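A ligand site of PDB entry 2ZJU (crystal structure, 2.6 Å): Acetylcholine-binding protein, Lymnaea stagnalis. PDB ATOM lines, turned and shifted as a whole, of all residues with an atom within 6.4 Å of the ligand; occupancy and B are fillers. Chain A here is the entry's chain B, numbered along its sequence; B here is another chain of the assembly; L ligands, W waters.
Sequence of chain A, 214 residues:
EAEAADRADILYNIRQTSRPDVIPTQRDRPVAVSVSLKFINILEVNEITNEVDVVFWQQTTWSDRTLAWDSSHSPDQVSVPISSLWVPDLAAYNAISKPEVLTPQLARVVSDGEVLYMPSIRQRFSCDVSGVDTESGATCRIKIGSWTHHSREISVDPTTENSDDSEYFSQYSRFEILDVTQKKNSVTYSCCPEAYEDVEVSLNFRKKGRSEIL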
ATOM      1  N   LYS A  38      29.480  17.406 -17.389  1.00  0.00           N
ATOM      2  CA  LYS A  38      30.709  18.184 -17.405  1.00  0.00           C
ATOM      3  C   LYS A  38      31.159  18.442 -15.961  1.00  0.00           C
ATOM      4  O   LYS A  38      30.813  19.437 -15.355  1.00  0.00           O
ATOM      5  CB  LYS A  38      30.468  19.518 -18.131  1.00  0.00           C
ATOM      6  CG  LYS A  38      30.436  19.380 -19.663  1.00  0.00           C
ATOM      7  CD  LYS A  38      31.789  18.869 -20.162  1.00  0.00           C
ATOM      8  CE  LYS A  38      31.882  18.714 -21.695  1.00  0.00           C
ATOM      9  NZ  LYS A  38      33.190  18.094 -22.126  1.00  0.00           N
ATOM     10  N   TRP A  57      27.792  19.983 -14.695  1.00  0.00           N
ATOM     11  CA  TRP A  57      26.768  20.579 -15.542  1.00  0.00           C
ATOM     12  C   TRP A  57      26.172  19.412 -16.298  1.00  0.00           C
ATOM     13  O   TRP A  57      26.863  18.717 -17.034  1.00  0.00           O
ATOM     14  CB  TRP A  57      27.390  21.540 -16.542  1.00  0.00           C
ATOM     15  CG  TRP A  57      28.149  22.629 -15.910  1.00  0.00           C
ATOM     16  CD1 TRP A  57      27.971  23.132 -14.661  1.00  0.00           C
ATOM     17  CD2 TRP A  57      29.155  23.428 -16.529  1.00  0.00           C
ATOM     18  NE1 TRP A  57      28.812  24.198 -14.444  1.00  0.00           N
ATOM     19  CE2 TRP A  57      29.554  24.406 -15.583  1.00  0.00           C
ATOM     20  CE3 TRP A  57      29.778  23.429 -17.783  1.00  0.00           C
ATOM     21  CZ2 TRP A  57      30.522  25.367 -15.845  1.00  0.00           C
ATOM     22  CZ3 TRP A  57      30.752  24.383 -18.056  1.00  0.00           C
ATOM     23  CH2 TRP A  57      31.122  25.341 -17.086  1.00  0.00           C
ATOM     24  N   GLN A  59      24.431  18.581 -19.149  1.00  0.00           N
ATOM     25  CA  GLN A  59      24.043  19.009 -20.487  1.00  0.00           C
ATOM     26  C   GLN A  59      23.009  18.035 -21.051  1.00  0.00           C
ATOM     27  O   GLN A  59      23.310  16.865 -21.280  1.00  0.00           O
ATOM     28  CB  GLN A  59      25.292  19.054 -21.379  1.00  0.00           C
ATOM     29  CG  GLN A  59      26.405  19.922 -20.779  1.00  0.00           C
ATOM     30  CD  GLN A  59      27.665  19.990 -21.643  1.00  0.00           C
ATOM     31  OE1 GLN A  59      28.382  18.986 -21.821  1.00  0.00           O
ATOM     32  NE2 GLN A  59      27.957  21.175 -22.162  1.00  0.00           N
ATOM     33  N   LEU A 106      16.529  27.568 -16.207  1.00  0.00           N
ATOM     34  CA  LEU A 106      16.040  27.983 -17.514  1.00  0.00           C
ATOM     35  C   LEU A 106      16.640  27.128 -18.626  1.00  0.00           C
ATOM     36  O   LEU A 106      17.818  26.715 -18.568  1.00  0.00           O
ATOM     37  CB  LEU A 106      16.437  29.445 -17.753  1.00  0.00           C
ATOM     38  CG  LEU A 106      16.102  30.441 -16.657  1.00  0.00           C
ATOM     39  CD1 LEU A 106      16.744  31.780 -16.973  1.00  0.00           C
ATOM     40  CD2 LEU A 106      14.600  30.582 -16.512  1.00  0.00           C
ATOM     41  N   ALA A 107      15.847  26.874 -19.653  1.00  0.00           N
ATOM     42  CA  ALA A 107      16.315  26.099 -20.795  1.00  0.00           C
ATOM     43  C   ALA A 107      16.465  26.999 -22.003  1.00  0.00           C
ATOM     44  O   ALA A 107      15.917  28.109 -22.052  1.00  0.00           O
ATOM     45  CB  ALA A 107      15.343  24.967 -21.106  1.00  0.00           C
ATOM     46  N   ARG A 108      17.200  26.507 -22.984  1.00  0.00           N
ATOM     47  CA  ARG A 108      17.425  27.225 -24.212  1.00  0.00           C
ATOM     48  C   ARG A 108      16.545  26.586 -25.299  1.00  0.00           C
ATOM     49  O   ARG A 108      16.671  25.384 -25.576  1.00  0.00           O
ATOM     50  CB  ARG A 108      18.892  27.119 -24.614  1.00  0.00           C
ATOM     51  CG  ARG A 108      19.311  28.172 -25.596  1.00  0.00           C
ATOM     52  CD  ARG A 108      19.277  29.569 -24.955  1.00  0.00           C
ATOM     53  NE  ARG A 108      19.602  30.572 -25.953  1.00  0.00           N
ATOM     54  CZ  ARG A 108      19.355  31.869 -25.842  1.00  0.00           C
ATOM     55  NH1 ARG A 108      18.765  32.357 -24.772  1.00  0.00           N
ATOM     56  NH2 ARG A 108      19.679  32.675 -26.852  1.00  0.00           N
ATOM     57  N   LEU A 116      17.518  22.844 -25.035  1.00  0.00           N
ATOM     58  CA  LEU A 116      18.756  22.562 -24.309  1.00  0.00           C
ATOM     59  C   LEU A 116      18.657  22.986 -22.853  1.00  0.00           C
ATOM     60  O   LEU A 116      18.253  24.109 -22.558  1.00  0.00           O
ATOM     61  CB  LEU A 116      19.934  23.272 -24.989  1.00  0.00           C
ATOM     62  CG  LEU A 116      21.209  23.297 -24.138  1.00  0.00           C
ATOM     63  CD1 LEU A 116      21.667  21.885 -23.775  1.00  0.00           C
ATOM     64  CD2 LEU A 116      22.281  24.046 -24.908  1.00  0.00           C
ATOM     65  N   TYR A 117      19.006  22.082 -21.950  1.00  0.00           N
ATOM     66  CA  TYR A 117      18.951  22.346 -20.514  1.00  0.00           C
ATOM     67  C   TYR A 117      20.275  21.896 -19.906  1.00  0.00           C
ATOM     68  O   TYR A 117      20.624  20.719 -19.958  1.00  0.00           O
ATOM     69  CB  TYR A 117      17.759  21.599 -19.881  1.00  0.00           C
ATOM     70  CG  TYR A 117      17.579  21.876 -18.407  1.00  0.00           C
ATOM     71  CD1 TYR A 117      17.602  23.168 -17.917  1.00  0.00           C
ATOM     72  CD2 TYR A 117      17.413  20.826 -17.499  1.00  0.00           C
ATOM     73  CE1 TYR A 117      17.471  23.433 -16.552  1.00  0.00           C
ATOM     74  CE2 TYR A 117      17.286  21.076 -16.125  1.00  0.00           C
ATOM     75  CZ  TYR A 117      17.316  22.388 -15.660  1.00  0.00           C
ATOM     76  OH  TYR A 117      17.205  22.683 -14.322  1.00  0.00           O
ATOM     77  N   MET A 118      21.021  22.846 -19.334  1.00  0.00           N
ATOM     78  CA  MET A 118      22.321  22.535 -18.765  1.00  0.00           C
ATOM     79  C   MET A 118      22.531  23.121 -17.377  1.00  0.00           C
ATOM     80  O   MET A 118      23.276  24.076 -17.187  1.00  0.00           O
ATOM     81  CB  MET A 118      23.406  23.060 -19.683  1.00  0.00           C
ATOM     82  CG  MET A 118      24.790  22.667 -19.264  1.00  0.00           C
ATOM     83  SD  MET A 118      25.950  23.222 -20.508  1.00  0.00           S
ATOM     84  CE  MET A 118      25.083  22.664 -22.040  1.00  0.00           C
ATOM     85  N   PRO A 119      21.897  22.520 -16.376  1.00  0.00           N
ATOM     86  CA  PRO A 119      22.015  22.981 -15.005  1.00  0.00           C
ATOM     87  C   PRO A 119      23.254  22.488 -14.281  1.00  0.00           C
ATOM     88  O   PRO A 119      23.730  21.359 -14.520  1.00  0.00           O
ATOM     89  CB  PRO A 119      20.767  22.419 -14.364  1.00  0.00           C
ATOM     90  CG  PRO A 119      20.697  21.058 -14.996  1.00  0.00           C
ATOM     91  CD  PRO A 119      20.930  21.406 -16.467  1.00  0.00           C
ATOM     92  N   TYR A 168      36.581  21.775 -17.767  1.00  0.00           N
ATOM     93  CA  TYR A 168      35.877  22.693 -16.882  1.00  0.00           C
ATOM     94  C   TYR A 168      36.087  22.389 -15.401  1.00  0.00           C
ATOM     95  O   TYR A 168      35.578  23.098 -14.532  1.00  0.00           O
ATOM     96  CB  TYR A 168      34.379  22.653 -17.223  1.00  0.00           C
ATOM     97  CG  TYR A 168      34.079  23.175 -18.607  1.00  0.00           C
ATOM     98  CD1 TYR A 168      34.443  24.460 -18.981  1.00  0.00           C
ATOM     99  CD2 TYR A 168      33.399  22.383 -19.537  1.00  0.00           C
ATOM    100  CE1 TYR A 168      34.160  24.969 -20.235  1.00  0.00           C
ATOM    101  CE2 TYR A 168      33.096  22.880 -20.820  1.00  0.00           C
ATOM    102  CZ  TYR A 168      33.476  24.174 -21.157  1.00  0.00           C
ATOM    103  OH  TYR A 168      33.173  24.697 -22.393  1.00  0.00           O
ATOM    104  N   TYR B  93      29.910  31.071 -11.433  1.00  0.00           N
ATOM    105  CA  TYR B  93      30.463  29.907 -12.082  1.00  0.00           C
ATOM    106  C   TYR B  93      31.205  28.944 -11.152  1.00  0.00           C
ATOM    107  O   TYR B  93      31.135  27.724 -11.335  1.00  0.00           O
ATOM    108  CB  TYR B  93      31.374  30.355 -13.225  1.00  0.00           C
ATOM    109  CG  TYR B  93      30.680  31.170 -14.303  1.00  0.00           C
ATOM    110  CD1 TYR B  93      31.404  31.998 -15.152  1.00  0.00           C
ATOM    111  CD2 TYR B  93      29.301  31.094 -14.496  1.00  0.00           C
ATOM    112  CE1 TYR B  93      30.781  32.735 -16.153  1.00  0.00           C
ATOM    113  CE2 TYR B  93      28.664  31.830 -15.493  1.00  0.00           C
ATOM    114  CZ  TYR B  93      29.408  32.650 -16.319  1.00  0.00           C
ATOM    115  OH  TYR B  93      28.767  33.383 -17.308  1.00  0.00           O
ATOM    116  N   SER B 146      25.561  35.947 -16.442  1.00  0.00           N
ATOM    117  CA  SER B 146      24.379  35.243 -16.914  1.00  0.00           C
ATOM    118  C   SER B 146      24.650  33.792 -17.252  1.00  0.00           C
ATOM    119  O   SER B 146      25.696  33.472 -17.812  1.00  0.00           O
ATOM    120  CB  SER B 146      23.784  35.913 -18.145  1.00  0.00           C
ATOM    121  OG  SER B 146      22.664  35.188 -18.610  1.00  0.00           O
ATOM    122  N   TRP B 147      23.699  32.928 -16.932  1.00  0.00           N
ATOM    123  CA  TRP B 147      23.838  31.500 -17.196  1.00  0.00           C
ATOM    124  C   TRP B 147      23.270  31.039 -18.554  1.00  0.00           C
ATOM    125  O   TRP B 147      23.748  30.065 -19.118  1.00  0.00           O
ATOM    126  CB  TRP B 147      23.202  30.718 -16.040  1.00  0.00           C
ATOM    127  CG  TRP B 147      23.426  29.258 -16.114  1.00  0.00           C
ATOM    128  CD1 TRP B 147      22.497  28.318 -16.427  1.00  0.00           C
ATOM    129  CD2 TRP B 147      24.642  28.562 -15.876  1.00  0.00           C
ATOM    130  NE1 TRP B 147      23.070  27.069 -16.401  1.00  0.00           N
ATOM    131  CE2 TRP B 147      24.384  27.188 -16.062  1.00  0.00           C
ATOM    132  CE3 TRP B 147      25.948  28.952 -15.528  1.00  0.00           C
ATOM    133  CZ2 TRP B 147      25.371  26.206 -15.912  1.00  0.00           C
ATOM    134  CZ3 TRP B 147      26.921  27.979 -15.371  1.00  0.00           C
ATOM    135  CH2 TRP B 147      26.629  26.629 -15.570  1.00  0.00           C
ATOM    136  N   THR B 148      22.262  31.732 -19.095  1.00  0.00           N
ATOM    137  CA  THR B 148      21.707  31.327 -20.399  1.00  0.00           C
ATOM    138  C   THR B 148      21.664  32.442 -21.452  1.00  0.00           C
ATOM    139  O   THR B 148      21.233  32.203 -22.579  1.00  0.00           O
ATOM    140  CB  THR B 148      20.281  30.742 -20.288  1.00  0.00           C
ATOM    141  OG1 THR B 148      19.388  31.729 -19.745  1.00  0.00           O
ATOM    142  CG2 THR B 148      20.281  29.499 -19.420  1.00  0.00           C
ATOM    143  N   TYR B 189      32.629  28.683 -24.786  1.00  0.00           N
ATOM    144  CA  TYR B 189      32.782  27.243 -24.588  1.00  0.00           C
ATOM    145  C   TYR B 189      33.270  26.526 -25.832  1.00  0.00           C
ATOM    146  O   TYR B 189      33.040  26.988 -26.946  1.00  0.00           O
ATOM    147  CB  TYR B 189      31.471  26.651 -24.110  1.00  0.00           C
ATOM    148  CG  TYR B 189      30.926  27.438 -22.951  1.00  0.00           C
ATOM    149  CD1 TYR B 189      30.006  28.465 -23.165  1.00  0.00           C
ATOM    150  CD2 TYR B 189      31.388  27.220 -21.663  1.00  0.00           C
ATOM    151  CE1 TYR B 189      29.573  29.262 -22.117  1.00  0.00           C
ATOM    152  CE2 TYR B 189      30.958  28.013 -20.602  1.00  0.00           C
ATOM    153  CZ  TYR B 189      30.049  29.027 -20.839  1.00  0.00           C
ATOM    154  OH  TYR B 189      29.612  29.793 -19.793  1.00  0.00           O
ATOM    155  N   SER B 190      33.966  25.416 -25.616  1.00  0.00           N
ATOM    156  CA  SER B 190      34.515  24.616 -26.704  1.00  0.00           C
ATOM    157  C   SER B 190      33.441  23.911 -27.529  1.00  0.00           C
ATOM    158  O   SER B 190      33.680  22.827 -28.074  1.00  0.00           O
ATOM    159  CB  SER B 190      35.521  23.581 -26.153  1.00  0.00           C
ATOM    160  OG  SER B 190      34.958  22.775 -25.133  1.00  0.00           O
ATOM    161  N   CYS B 191      32.271  24.532 -27.604  1.00  0.00           N
ATOM    162  CA  CYS B 191      31.146  23.971 -28.360  1.00  0.00           C
ATOM    163  C   CYS B 191      30.603  24.973 -29.323  1.00  0.00           C
ATOM    164  O   CYS B 191      30.429  24.724 -30.516  1.00  0.00           O
ATOM    165  CB  CYS B 191      29.973  23.633 -27.440  1.00  0.00           C
ATOM    166  SG  CYS B 191      29.070  25.039 -26.638  1.00  0.00           S
ATOM    167  N   CYS B 192      30.351  26.118 -28.739  1.00  0.00           N
ATOM    168  CA  CYS B 192      29.700  27.195 -29.409  1.00  0.00           C
ATOM    169  C   CYS B 192      30.549  28.462 -29.436  1.00  0.00           C
ATOM    170  O   CYS B 192      31.342  28.717 -28.532  1.00  0.00           O
ATOM    171  CB  CYS B 192      28.389  27.381 -28.670  1.00  0.00           C
ATOM    172  SG  CYS B 192      27.715  25.805 -27.978  1.00  0.00           S
ATOM    173  N   TYR B 196      29.824  34.384 -23.033  1.00  0.00           N
ATOM    174  CA  TYR B 196      28.949  34.892 -21.987  1.00  0.00           C
ATOM    175  C   TYR B 196      29.698  35.817 -21.038  1.00  0.00           C
ATOM    176  O   TYR B 196      30.485  35.381 -20.219  1.00  0.00           O
ATOM    177  CB  TYR B 196      28.348  33.725 -21.185  1.00  0.00           C
ATOM    178  CG  TYR B 196      27.444  32.805 -21.982  1.00  0.00           C
ATOM    179  CD1 TYR B 196      27.939  32.079 -23.077  1.00  0.00           C
ATOM    180  CD2 TYR B 196      26.101  32.644 -21.651  1.00  0.00           C
ATOM    181  CE1 TYR B 196      27.105  31.209 -23.799  1.00  0.00           C
ATOM    182  CE2 TYR B 196      25.266  31.783 -22.370  1.00  0.00           C
ATOM    183  CZ  TYR B 196      25.772  31.080 -23.436  1.00  0.00           C
ATOM    184  OH  TYR B 196      24.951  30.240 -24.152  1.00  0.00           O
HETATM  185  C1  LIG L   1      23.641  27.458 -22.671  1.00  0.00           C
HETATM  186  C2  LIG L   1      22.319  26.930 -22.684  1.00  0.00           C
HETATM  187  C3  LIG L   1      21.773  26.464 -21.453  1.00  0.00           C
HETATM  188 CL1  LIG L   1      20.161  25.815 -21.421  1.00  0.00          CL
HETATM  189  N1  LIG L   1      22.483  26.519 -20.317  1.00  0.00           N
HETATM  190  C4  LIG L   1      23.736  27.013 -20.274  1.00  0.00           C
HETATM  191  C5  LIG L   1      24.376  27.518 -21.455  1.00  0.00           C
HETATM  192  C6  LIG L   1      25.805  28.090 -21.433  1.00  0.00           C
HETATM  193  N2  LIG L   1      26.798  27.414 -20.573  1.00  0.00           N
HETATM  194  C7  LIG L   1      27.030  27.791 -19.161  1.00  0.00           C
HETATM  195  C8  LIG L   1      28.132  26.848 -18.652  1.00  0.00           C
HETATM  196  N3  LIG L   1      28.479  25.994 -19.788  1.00  0.00           N
HETATM  197  C9  LIG L   1      27.671  26.331 -20.904  1.00  0.00           C
HETATM  198  N4  LIG L   1      27.742  25.791 -22.060  1.00  0.00           N
HETATM  199  N5  LIG L   1      28.479  24.757 -22.607  1.00  0.00           N
HETATM  200  O1  LIG L   1      29.380  24.094 -21.949  1.00  0.00           O
HETATM  201  O2  LIG L   1      28.268  24.443 -23.834  1.00  0.00           O
HETATM  202  O   HOH W   1      27.514  30.891 -18.371  1.00  0.00           O
HETATM  203  O   HOH W   2      20.686  25.567 -18.235  1.00  0.00           O
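O1 of the ligand lies within hydrogen-bond range of NE2 of Gln 59 (3.3 Å).
The side-chain sulfur (SD) of Met 118 sits close to a nitrogen (N4) of the ligand.
The backbone carbonyl oxygen (O) of Leu 116 sits at hydrogen-bond distance from the backbone NH (N) of Arg 108 (2.7 Å).
The side-chain sulfur (SG) of Cys 191 of chain B is disulfide-bonded to the side-chain sulfur (SG) of Cys 192 of chain B (2.1 Å).
The side-chain amide nitrogen (NE2) of Gln 59 sits close to the side-chain sulfur (SD) of Met 118, at 3.3 Å.
O of Met 118 is in hydrogen-bond range of NE1 of Trp 147 of chain B (3.1 Å).
The backbone carbonyl oxygen (O) of Trp 57 lies within hydrogen-bond range of the backbone NH (N) of Lys 38, at 2.9 Å.
NH1 of Arg 108 sits at hydrogen-bond distance from O of Thr 148 of chain B, 3.3 Å away.
OH of Tyr 168 sits at hydrogen-bond distance from N of Ser 190 of chain B (3.4 Å).
The side-chain sulfur (SG) of Cys 191 of chain B lies close to an oxygen (O2) of the ligand.
Trp 57 touches the ligand (CZ3 to N3, 3.3 Å).
O of Leu 106 touches CL1 of the ligand, at 3.8 Å.
CA of Ala 107 touches CL1 of the ligand (3.9 Å).
Arg 108 touches the ligand.
Leu 116 touches the ligand (O to CL1, 2.8 Å).
Tyr 117 touches the ligand (CA to CL1, 3.8 Å).
Tyr 168 touches the ligand (OH to O1, 3.9 Å).
Trp 147 of chain B touches the ligand (O to C4, 3.3 Å).
CG2 of Thr 148 of chain B touches N1 of the ligand (3.8 Å).
CE2 of Tyr 189 of chain B touches N3 of the ligand, at 3.3 Å.
Tyr 196 of chain B touches the ligand (OH to C1, 3.4 Å).
Hydrophobic or aromatic side chains within 4 Å of the ligand: Trp 57, Leu 116, Met 118, Trp 147 of chain B, Tyr 189 of chain B and Tyr 196 of chain B.
The nearest printed residue that does not touch the ligand is Cys 192 of chain B (4.4 Å).
Water W2 lies within hydrogen-bond range of N1 of the ligand, N of Met 118, O of Leu 106 and NE1 of Trp 147 of chain B.
Water W1 lies within hydrogen-bond range of OH of Tyr 189 of chain B (2.8 Å), OH of Tyr 93 of chain B (3.0 Å) and O of Ser 146 of chain B (3.2 Å).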
